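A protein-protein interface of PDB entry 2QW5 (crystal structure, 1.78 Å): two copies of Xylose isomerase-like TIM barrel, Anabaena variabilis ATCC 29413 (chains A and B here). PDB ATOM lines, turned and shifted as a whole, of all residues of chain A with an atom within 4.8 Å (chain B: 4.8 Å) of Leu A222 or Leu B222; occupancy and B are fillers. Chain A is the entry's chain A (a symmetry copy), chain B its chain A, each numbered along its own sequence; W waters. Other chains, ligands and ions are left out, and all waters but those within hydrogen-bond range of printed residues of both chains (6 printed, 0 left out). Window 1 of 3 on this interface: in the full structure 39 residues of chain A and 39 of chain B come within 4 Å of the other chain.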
ATOM      1  N   THR A 186     -29.075 -11.844   2.880  1.00  0.00           N
ATOM      2  CA  THR A 186     -28.534 -10.636   2.286  1.00  0.00           C
ATOM      3  C   THR A 186     -29.538  -9.842   1.475  1.00  0.00           C
ATOM      4  O   THR A 186     -30.423 -10.413   0.838  1.00  0.00           O
ATOM      5  CB  THR A 186     -27.298 -10.921   1.371  1.00  0.00           C
ATOM      6  OG1 THR A 186     -26.819  -9.679   0.831  1.00  0.00           O
ATOM      7  CG2 THR A 186     -27.610 -11.876   0.210  1.00  0.00           C
ATOM      8  N   TRP A 188     -29.017  -8.499  -1.242  1.00  0.00           N
ATOM      9  CA  TRP A 188     -28.917  -8.930  -2.628  1.00  0.00           C
ATOM     10  C   TRP A 188     -30.003  -9.902  -3.042  1.00  0.00           C
ATOM     11  O   TRP A 188     -30.372  -9.907  -4.221  1.00  0.00           O
ATOM     12  CB  TRP A 188     -27.546  -9.521  -2.946  1.00  0.00           C
ATOM     13  CG  TRP A 188     -26.477  -8.505  -3.174  1.00  0.00           C
ATOM     14  CD1 TRP A 188     -25.406  -8.286  -2.399  1.00  0.00           C
ATOM     15  CD2 TRP A 188     -26.384  -7.562  -4.260  1.00  0.00           C
ATOM     16  NE1 TRP A 188     -24.636  -7.286  -2.920  1.00  0.00           N
ATOM     17  CE2 TRP A 188     -25.198  -6.839  -4.081  1.00  0.00           C
ATOM     18  CE3 TRP A 188     -27.171  -7.285  -5.382  1.00  0.00           C
ATOM     19  CZ2 TRP A 188     -24.791  -5.820  -4.964  1.00  0.00           C
ATOM     20  CZ3 TRP A 188     -26.740  -6.295  -6.286  1.00  0.00           C
ATOM     21  CH2 TRP A 188     -25.569  -5.570  -6.049  1.00  0.00           C
ATOM     22  N   ALA A 218     -22.325 -16.703   5.045  1.00  0.00           N
ATOM     23  CA  ALA A 218     -22.406 -15.879   3.804  1.00  0.00           C
ATOM     24  C   ALA A 218     -23.265 -14.631   4.031  1.00  0.00           C
ATOM     25  O   ALA A 218     -22.832 -13.514   3.704  1.00  0.00           O
ATOM     26  CB  ALA A 218     -22.972 -16.682   2.637  1.00  0.00           C
ATOM     27  N   HIS A 219     -24.446 -14.817   4.633  1.00  0.00           N
ATOM     28  CA  HIS A 219     -25.344 -13.673   4.960  1.00  0.00           C
ATOM     29  C   HIS A 219     -24.796 -12.779   6.041  1.00  0.00           C
ATOM     30  O   HIS A 219     -24.963 -11.533   5.941  1.00  0.00           O
ATOM     31  CB  HIS A 219     -26.770 -14.106   5.280  1.00  0.00           C
ATOM     32  CG  HIS A 219     -27.396 -14.918   4.199  1.00  0.00           C
ATOM     33  ND1 HIS A 219     -27.385 -14.527   2.879  1.00  0.00           N
ATOM     34  CD2 HIS A 219     -28.056 -16.094   4.244  1.00  0.00           C
ATOM     35  CE1 HIS A 219     -27.976 -15.460   2.148  1.00  0.00           C
ATOM     36  NE2 HIS A 219     -28.444 -16.392   2.960  1.00  0.00           N
ATOM     37  N   GLU A 220     -24.108 -13.353   7.029  1.00  0.00           N
ATOM     38  CA  GLU A 220     -23.505 -12.544   8.122  1.00  0.00           C
ATOM     39  C   GLU A 220     -22.402 -11.622   7.592  1.00  0.00           C
ATOM     40  O   GLU A 220     -22.379 -10.423   7.877  1.00  0.00           O
ATOM     41  CB  GLU A 220     -22.964 -13.429   9.246  1.00  0.00           C
ATOM     42  CG  GLU A 220     -22.360 -12.660  10.453  1.00  0.00           C
ATOM     43  CD  GLU A 220     -23.328 -11.681  11.061  1.00  0.00           C
ATOM     44  OE1 GLU A 220     -24.527 -12.012  11.106  1.00  0.00           O
ATOM     45  OE2 GLU A 220     -22.889 -10.591  11.501  1.00  0.00           O
ATOM     46  N   ILE A 221     -21.542 -12.168   6.741  1.00  0.00           N
ATOM     47  CA  ILE A 221     -20.452 -11.401   6.152  1.00  0.00           C
ATOM     48  C   ILE A 221     -20.967 -10.321   5.202  1.00  0.00           C
ATOM     49  O   ILE A 221     -20.471  -9.188   5.272  1.00  0.00           O
ATOM     50  CB  ILE A 221     -19.473 -12.312   5.418  1.00  0.00           C
ATOM     51  CG1 ILE A 221     -18.618 -13.134   6.393  1.00  0.00           C
ATOM     52  CG2 ILE A 221     -18.446 -11.437   4.588  1.00  0.00           C
ATOM     53  CD1 ILE A 221     -19.138 -13.428   7.887  1.00  0.00           C
ATOM     54  N   LEU A 222     -21.925 -10.664   4.318  1.00  0.00           N
ATOM     55  CA  LEU A 222     -22.440  -9.700   3.328  1.00  0.00           C
ATOM     56  C   LEU A 222     -23.147  -8.513   3.943  1.00  0.00           C
ATOM     57  O   LEU A 222     -23.034  -7.413   3.400  1.00  0.00           O
ATOM     58  CB  LEU A 222     -23.340 -10.335   2.250  1.00  0.00           C
ATOM     59  CG  LEU A 222     -22.601 -10.746   0.955  1.00  0.00           C
ATOM     60  CD1 LEU A 222     -21.427 -11.682   1.260  1.00  0.00           C
ATOM     61  CD2 LEU A 222     -23.554 -11.321  -0.139  1.00  0.00           C
ATOM     62  N   ASP A 223     -23.906  -8.730   5.017  1.00  0.00           N
ATOM     63  CA  ASP A 223     -24.717  -7.650   5.646  1.00  0.00           C
ATOM     64  C   ASP A 223     -24.478  -7.321   7.117  1.00  0.00           C
ATOM     65  O   ASP A 223     -24.982  -6.279   7.593  1.00  0.00           O
ATOM     66  CB  ASP A 223     -26.227  -7.957   5.484  1.00  0.00           C
ATOM     67  CG  ASP A 223     -26.692  -7.918   4.049  1.00  0.00           C
ATOM     68  OD1 ASP A 223     -25.976  -8.434   3.162  1.00  0.00           O
ATOM     69  OD2 ASP A 223     -27.786  -7.357   3.795  1.00  0.00           O
ATOM     70  N   GLY A 224     -23.753  -8.172   7.832  1.00  0.00           N
ATOM     71  CA  GLY A 224     -23.584  -8.010   9.275  1.00  0.00           C
ATOM     72  C   GLY A 224     -22.684  -6.884   9.722  1.00  0.00           C
ATOM     73  O   GLY A 224     -21.978  -6.263   8.940  1.00  0.00           O
ATOM     74  N   PRO A 251     -18.841 -16.364   0.793  1.00  0.00           N
ATOM     75  CA  PRO A 251     -19.592 -15.197   0.242  1.00  0.00           C
ATOM     76  C   PRO A 251     -20.198 -15.364  -1.151  1.00  0.00           C
ATOM     77  O   PRO A 251     -21.306 -14.881  -1.392  1.00  0.00           O
ATOM     78  CB  PRO A 251     -18.530 -14.097   0.219  1.00  0.00           C
ATOM     79  CG  PRO A 251     -17.659 -14.446   1.414  1.00  0.00           C
ATOM     80  CD  PRO A 251     -17.514 -15.950   1.288  1.00  0.00           C
ATOM     81  N   ASP A 252     -19.496 -16.081  -2.041  1.00  0.00           N
ATOM     82  CA  ASP A 252     -20.012 -16.312  -3.391  1.00  0.00           C
ATOM     83  C   ASP A 252     -20.954 -17.519  -3.491  1.00  0.00           C
ATOM     84  O   ASP A 252     -21.436 -17.801  -4.567  1.00  0.00           O
ATOM     85  CB  ASP A 252     -18.875 -16.378  -4.424  1.00  0.00           C
ATOM     86  CG  ASP A 252     -18.272 -17.776  -4.594  1.00  0.00           C
ATOM     87  OD1 ASP A 252     -18.385 -18.616  -3.691  1.00  0.00           O
ATOM     88  OD2 ASP A 252     -17.665 -18.001  -5.670  1.00  0.00           O
ATOM     89  N   THR B 186     -17.811  -7.636  -8.206  1.00  0.00           N
ATOM     90  CA  THR B 186     -18.624  -8.789  -7.867  1.00  0.00           C
ATOM     91  C   THR B 186     -19.623  -9.178  -8.937  1.00  0.00           C
ATOM     92  O   THR B 186     -20.160  -8.319  -9.637  1.00  0.00           O
ATOM     93  CB  THR B 186     -19.408  -8.595  -6.528  1.00  0.00           C
ATOM     94  OG1 THR B 186     -20.178  -9.779  -6.260  1.00  0.00           O
ATOM     95  CG2 THR B 186     -20.354  -7.386  -6.548  1.00  0.00           C
ATOM     96  N   TRP B 188     -22.538 -10.036  -8.470  1.00  0.00           N
ATOM     97  CA  TRP B 188     -23.798  -9.371  -8.173  1.00  0.00           C
ATOM     98  C   TRP B 188     -24.041  -8.130  -9.007  1.00  0.00           C
ATOM     99  O   TRP B 188     -25.207  -7.815  -9.270  1.00  0.00           O
ATOM    100  CB  TRP B 188     -23.929  -9.031  -6.691  1.00  0.00           C
ATOM    101  CG  TRP B 188     -24.323 -10.184  -5.828  1.00  0.00           C
ATOM    102  CD1 TRP B 188     -23.569 -10.771  -4.889  1.00  0.00           C
ATOM    103  CD2 TRP B 188     -25.579 -10.891  -5.834  1.00  0.00           C
ATOM    104  NE1 TRP B 188     -24.257 -11.788  -4.291  1.00  0.00           N
ATOM    105  CE2 TRP B 188     -25.508 -11.868  -4.833  1.00  0.00           C
ATOM    106  CE3 TRP B 188     -26.764 -10.770  -6.565  1.00  0.00           C
ATOM    107  CZ2 TRP B 188     -26.568 -12.756  -4.564  1.00  0.00           C
ATOM    108  CZ3 TRP B 188     -27.838 -11.630  -6.265  1.00  0.00           C
ATOM    109  CH2 TRP B 188     -27.712 -12.617  -5.284  1.00  0.00           C
ATOM    110  N   ALA B 218     -14.406  -4.830  -0.831  1.00  0.00           N
ATOM    111  CA  ALA B 218     -15.794  -5.356  -0.970  1.00  0.00           C
ATOM    112  C   ALA B 218     -15.868  -6.416  -2.075  1.00  0.00           C
ATOM    113  O   ALA B 218     -16.405  -7.512  -1.846  1.00  0.00           O
ATOM    114  CB  ALA B 218     -16.788  -4.238  -1.268  1.00  0.00           C
ATOM    115  N   HIS B 219     -15.289  -6.108  -3.242  1.00  0.00           N
ATOM    116  CA  HIS B 219     -15.246  -7.080  -4.372  1.00  0.00           C
ATOM    117  C   HIS B 219     -14.356  -8.264  -4.102  1.00  0.00           C
ATOM    118  O   HIS B 219     -14.722  -9.402  -4.503  1.00  0.00           O
ATOM    119  CB  HIS B 219     -14.899  -6.429  -5.705  1.00  0.00           C
ATOM    120  CG  HIS B 219     -15.809  -5.306  -6.067  1.00  0.00           C
ATOM    121  ND1 HIS B 219     -17.181  -5.422  -6.025  1.00  0.00           N
ATOM    122  CD2 HIS B 219     -15.545  -4.050  -6.483  1.00  0.00           C
ATOM    123  CE1 HIS B 219     -17.722  -4.260  -6.358  1.00  0.00           C
ATOM    124  NE2 HIS B 219     -16.752  -3.429  -6.698  1.00  0.00           N
ATOM    125  N   GLU B 220     -13.243  -8.055  -3.398  1.00  0.00           N
ATOM    126  CA  GLU B 220     -12.321  -9.172  -3.059  1.00  0.00           C
ATOM    127  C   GLU B 220     -12.988 -10.182  -2.120  1.00  0.00           C
ATOM    128  O   GLU B 220     -12.961 -11.391  -2.357  1.00  0.00           O
ATOM    129  CB  GLU B 220     -11.016  -8.660  -2.448  1.00  0.00           C
ATOM    130  CG  GLU B 220      -9.974  -9.761  -2.110  1.00  0.00           C
ATOM    131  CD  GLU B 220      -9.624 -10.616  -3.298  1.00  0.00           C
ATOM    132  OE1 GLU B 220      -9.559 -10.055  -4.408  1.00  0.00           O
ATOM    133  OE2 GLU B 220      -9.406 -11.838  -3.121  1.00  0.00           O
ATOM    134  N   ILE B 221     -13.671  -9.671  -1.101  1.00  0.00           N
ATOM    135  CA  ILE B 221     -14.364 -10.518  -0.140  1.00  0.00           C
ATOM    136  C   ILE B 221     -15.539 -11.257  -0.777  1.00  0.00           C
ATOM    137  O   ILE B 221     -15.690 -12.460  -0.523  1.00  0.00           O
ATOM    138  CB  ILE B 221     -14.850  -9.707   1.057  1.00  0.00           C
ATOM    139  CG1 ILE B 221     -13.691  -9.292   1.974  1.00  0.00           C
ATOM    140  CG2 ILE B 221     -15.804 -10.597   1.956  1.00  0.00           C
ATOM    141  CD1 ILE B 221     -12.190  -9.197   1.401  1.00  0.00           C
ATOM    142  N   LEU B 222     -16.369 -10.552  -1.573  1.00  0.00           N
ATOM    143  CA  LEU B 222     -17.560 -11.172  -2.185  1.00  0.00           C
ATOM    144  C   LEU B 222     -17.237 -12.281  -3.161  1.00  0.00           C
ATOM    145  O   LEU B 222     -17.993 -13.251  -3.223  1.00  0.00           O
ATOM    146  CB  LEU B 222     -18.515 -10.162  -2.850  1.00  0.00           C
ATOM    147  CG  LEU B 222     -19.664  -9.668  -1.940  1.00  0.00           C
ATOM    148  CD1 LEU B 222     -19.123  -9.079  -0.633  1.00  0.00           C
ATOM    149  CD2 LEU B 222     -20.650  -8.701  -2.667  1.00  0.00           C
ATOM    150  N   ASP B 223     -16.172 -12.126  -3.947  1.00  0.00           N
ATOM    151  CA  ASP B 223     -15.817 -13.114  -5.005  1.00  0.00           C
ATOM    152  C   ASP B 223     -14.439 -13.769  -4.958  1.00  0.00           C
ATOM    153  O   ASP B 223     -14.214 -14.755  -5.695  1.00  0.00           O
ATOM    154  CB  ASP B 223     -15.971 -12.470  -6.406  1.00  0.00           C
ATOM    155  CG  ASP B 223     -17.400 -12.127  -6.750  1.00  0.00           C
ATOM    156  OD1 ASP B 223     -18.128 -11.608  -5.875  1.00  0.00           O
ATOM    157  OD2 ASP B 223     -17.809 -12.384  -7.908  1.00  0.00           O
ATOM    158  N   GLY B 224     -13.534 -13.248  -4.141  1.00  0.00           N
ATOM    159  CA  GLY B 224     -12.150 -13.723  -4.127  1.00  0.00           C
ATOM    160  C   GLY B 224     -11.915 -15.080  -3.506  1.00  0.00           C
ATOM    161  O   GLY B 224     -12.781 -15.668  -2.875  1.00  0.00           O
ATOM    162  N   PRO B 251     -18.491  -5.047   2.856  1.00  0.00           N
ATOM    163  CA  PRO B 251     -19.304  -5.897   1.937  1.00  0.00           C
ATOM    164  C   PRO B 251     -20.654  -5.335   1.493  1.00  0.00           C
ATOM    165  O   PRO B 251     -21.035  -5.517   0.335  1.00  0.00           O
ATOM    166  CB  PRO B 251     -19.516  -7.169   2.759  1.00  0.00           C
ATOM    167  CG  PRO B 251     -18.241  -7.255   3.580  1.00  0.00           C
ATOM    168  CD  PRO B 251     -18.041  -5.820   4.030  1.00  0.00           C
ATOM    169  N   ASP B 252     -21.345  -4.621   2.394  1.00  0.00           N
ATOM    170  CA  ASP B 252     -22.635  -4.025   2.047  1.00  0.00           C
ATOM    171  C   ASP B 252     -22.517  -2.650   1.373  1.00  0.00           C
ATOM    172  O   ASP B 252     -23.528  -2.067   1.046  1.00  0.00           O
ATOM    173  CB  ASP B 252     -23.586  -3.997   3.256  1.00  0.00           C
ATOM    174  CG  ASP B 252     -23.434  -2.751   4.134  1.00  0.00           C
ATOM    175  OD1 ASP B 252     -22.380  -2.101   4.116  1.00  0.00           O
ATOM    176  OD2 ASP B 252     -24.414  -2.451   4.860  1.00  0.00           O
HETATM  177  O   HOH W   1     -26.282  -3.915   6.158  1.00  0.00           O
HETATM  178  O   HOH W   2     -20.862 -12.869  -3.710  1.00  0.00           O
HETATM  179  O   HOH W   3     -16.165 -16.462  -7.314  1.00  0.00           O
HETATM  180  O   HOH W   4     -23.536 -14.462  -2.874  1.00  0.00           O
HETATM  181  O   HOH W   5     -23.705  -7.079   0.563  1.00  0.00           O
HETATM  182  O   HOH W   6     -22.660  -5.157  -1.804  1.00  0.00           O
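Water W3 bridges the side-chain carboxylate of Asp A252 (2.7 Å) and the backbone carbonyl oxygen of Asp B223 (3.1 Å).
Water W1 bridges the side-chain carboxylate (OD2) of Asp B252 (2.7 Å) and the backbone carbonyl oxygen (O) of Asp A223 (3.1 Å).
Water W6 lies within hydrogen-bond range of the backbone carbonyl oxygen of Pro B251 (2.7 Å) and the indole nitrogen of Trp A188 (3.1 Å).
Water W4 bridges O of Pro A251 (2.7 Å) and NE1 of Trp B188 (3.1 Å).
Water W2 bridges the backbone carbonyl oxygen of Leu B222 and the backbone carbonyl oxygen of Pro A251.
Water W5 lies within hydrogen-bond range of O of Leu A222 (2.9 Å) and O of Pro B251 (3.1 Å).
The backbone NH of Trp B188 sits close to the side-chain hydroxyl of Thr B186, at 3.2 Å.
The side-chain hydroxyl (OG1) of Thr A186 sits close to the backbone NH (N) of Trp A188, at 3.2 Å.
Of the 11 printed residues of chain A, 5 touch a printed residue of chain B.
Printed residues of chain A that touch a printed residue of chain B: Trp A188, Ile A221, Leu A222, Pro A251 and Asp A252.
Hydrophobic or aromatic side chains of chain A that line the printed part of chain B: Trp A188, Ile A221, Leu A222 and Pro A251.
Along chain A the printed residues that touch a printed residue of chain B span positions 188 to 252.
Of the 11 printed residues of chain B, 5 touch a printed residue of chain A.
Hydrophobic or aromatic side chains of chain B that line the printed part of chain A: Trp B188, Ile B221, Leu B222 and Pro B251.
Among the printed residues, no Asp or Glu carboxylate lies within 4 Å of a Lys or Arg side-chain nitrogen of the other chain.
Ala A218 touches none of the printed residues of chain B.
Of the printed residues of chain B, Ile A221 touches Ile B221 (3.8 Å) and Pro B251 (3.4 Å).
Leu B222 touches three residues of chain A.
Asp B223 touches none of the printed residues of chain A.
Printed residues of chain A within 4 Å of Asp B252: Leu A222 (3.4 Å).
The nearest residue of chain B that does not touch Leu A222 is Trp B188 (4.2 Å).
The nearest residue of chain A that does not touch Leu B222 is Trp A188 (4.2 Å).
The nearest printed residue of chain B that does not touch Asp A252 is Asp B223 (4.5 Å).
Trp A188 touches its own counterpart, Trp B188.
Ile B221 touches its own counterpart, Ile A221.
Ile A221 touches Pro B251, and with the chains exchanged Pro A251 touches Ile B221.
Leu B222 touches its own counterpart, Leu A222.
11 positions are printed for both chains.
The backbone NH (N) of Asp A252 sits at hydrogen-bond distance from the backbone carbonyl oxygen (O) of Leu B222, at 3.4 Å.
N of Asp B252 lies within hydrogen-bond range of O of Leu A222, 3.4 Å away.
Among the printed residues, merely in contact across the chains: Trp A188 with Trp B188 (3.6 Å), Ile A221 with Ile B221 (3.8 Å), Ile A221 with Pro B251 (3.4 Å), Leu A222 with Leu B222 (3.96 Å), Leu A222 with Pro B251 (3.6 Å), Pro A251 with Ile B221 (3.4 Å) and Pro A251 with Leu B222 (3.6 Å).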
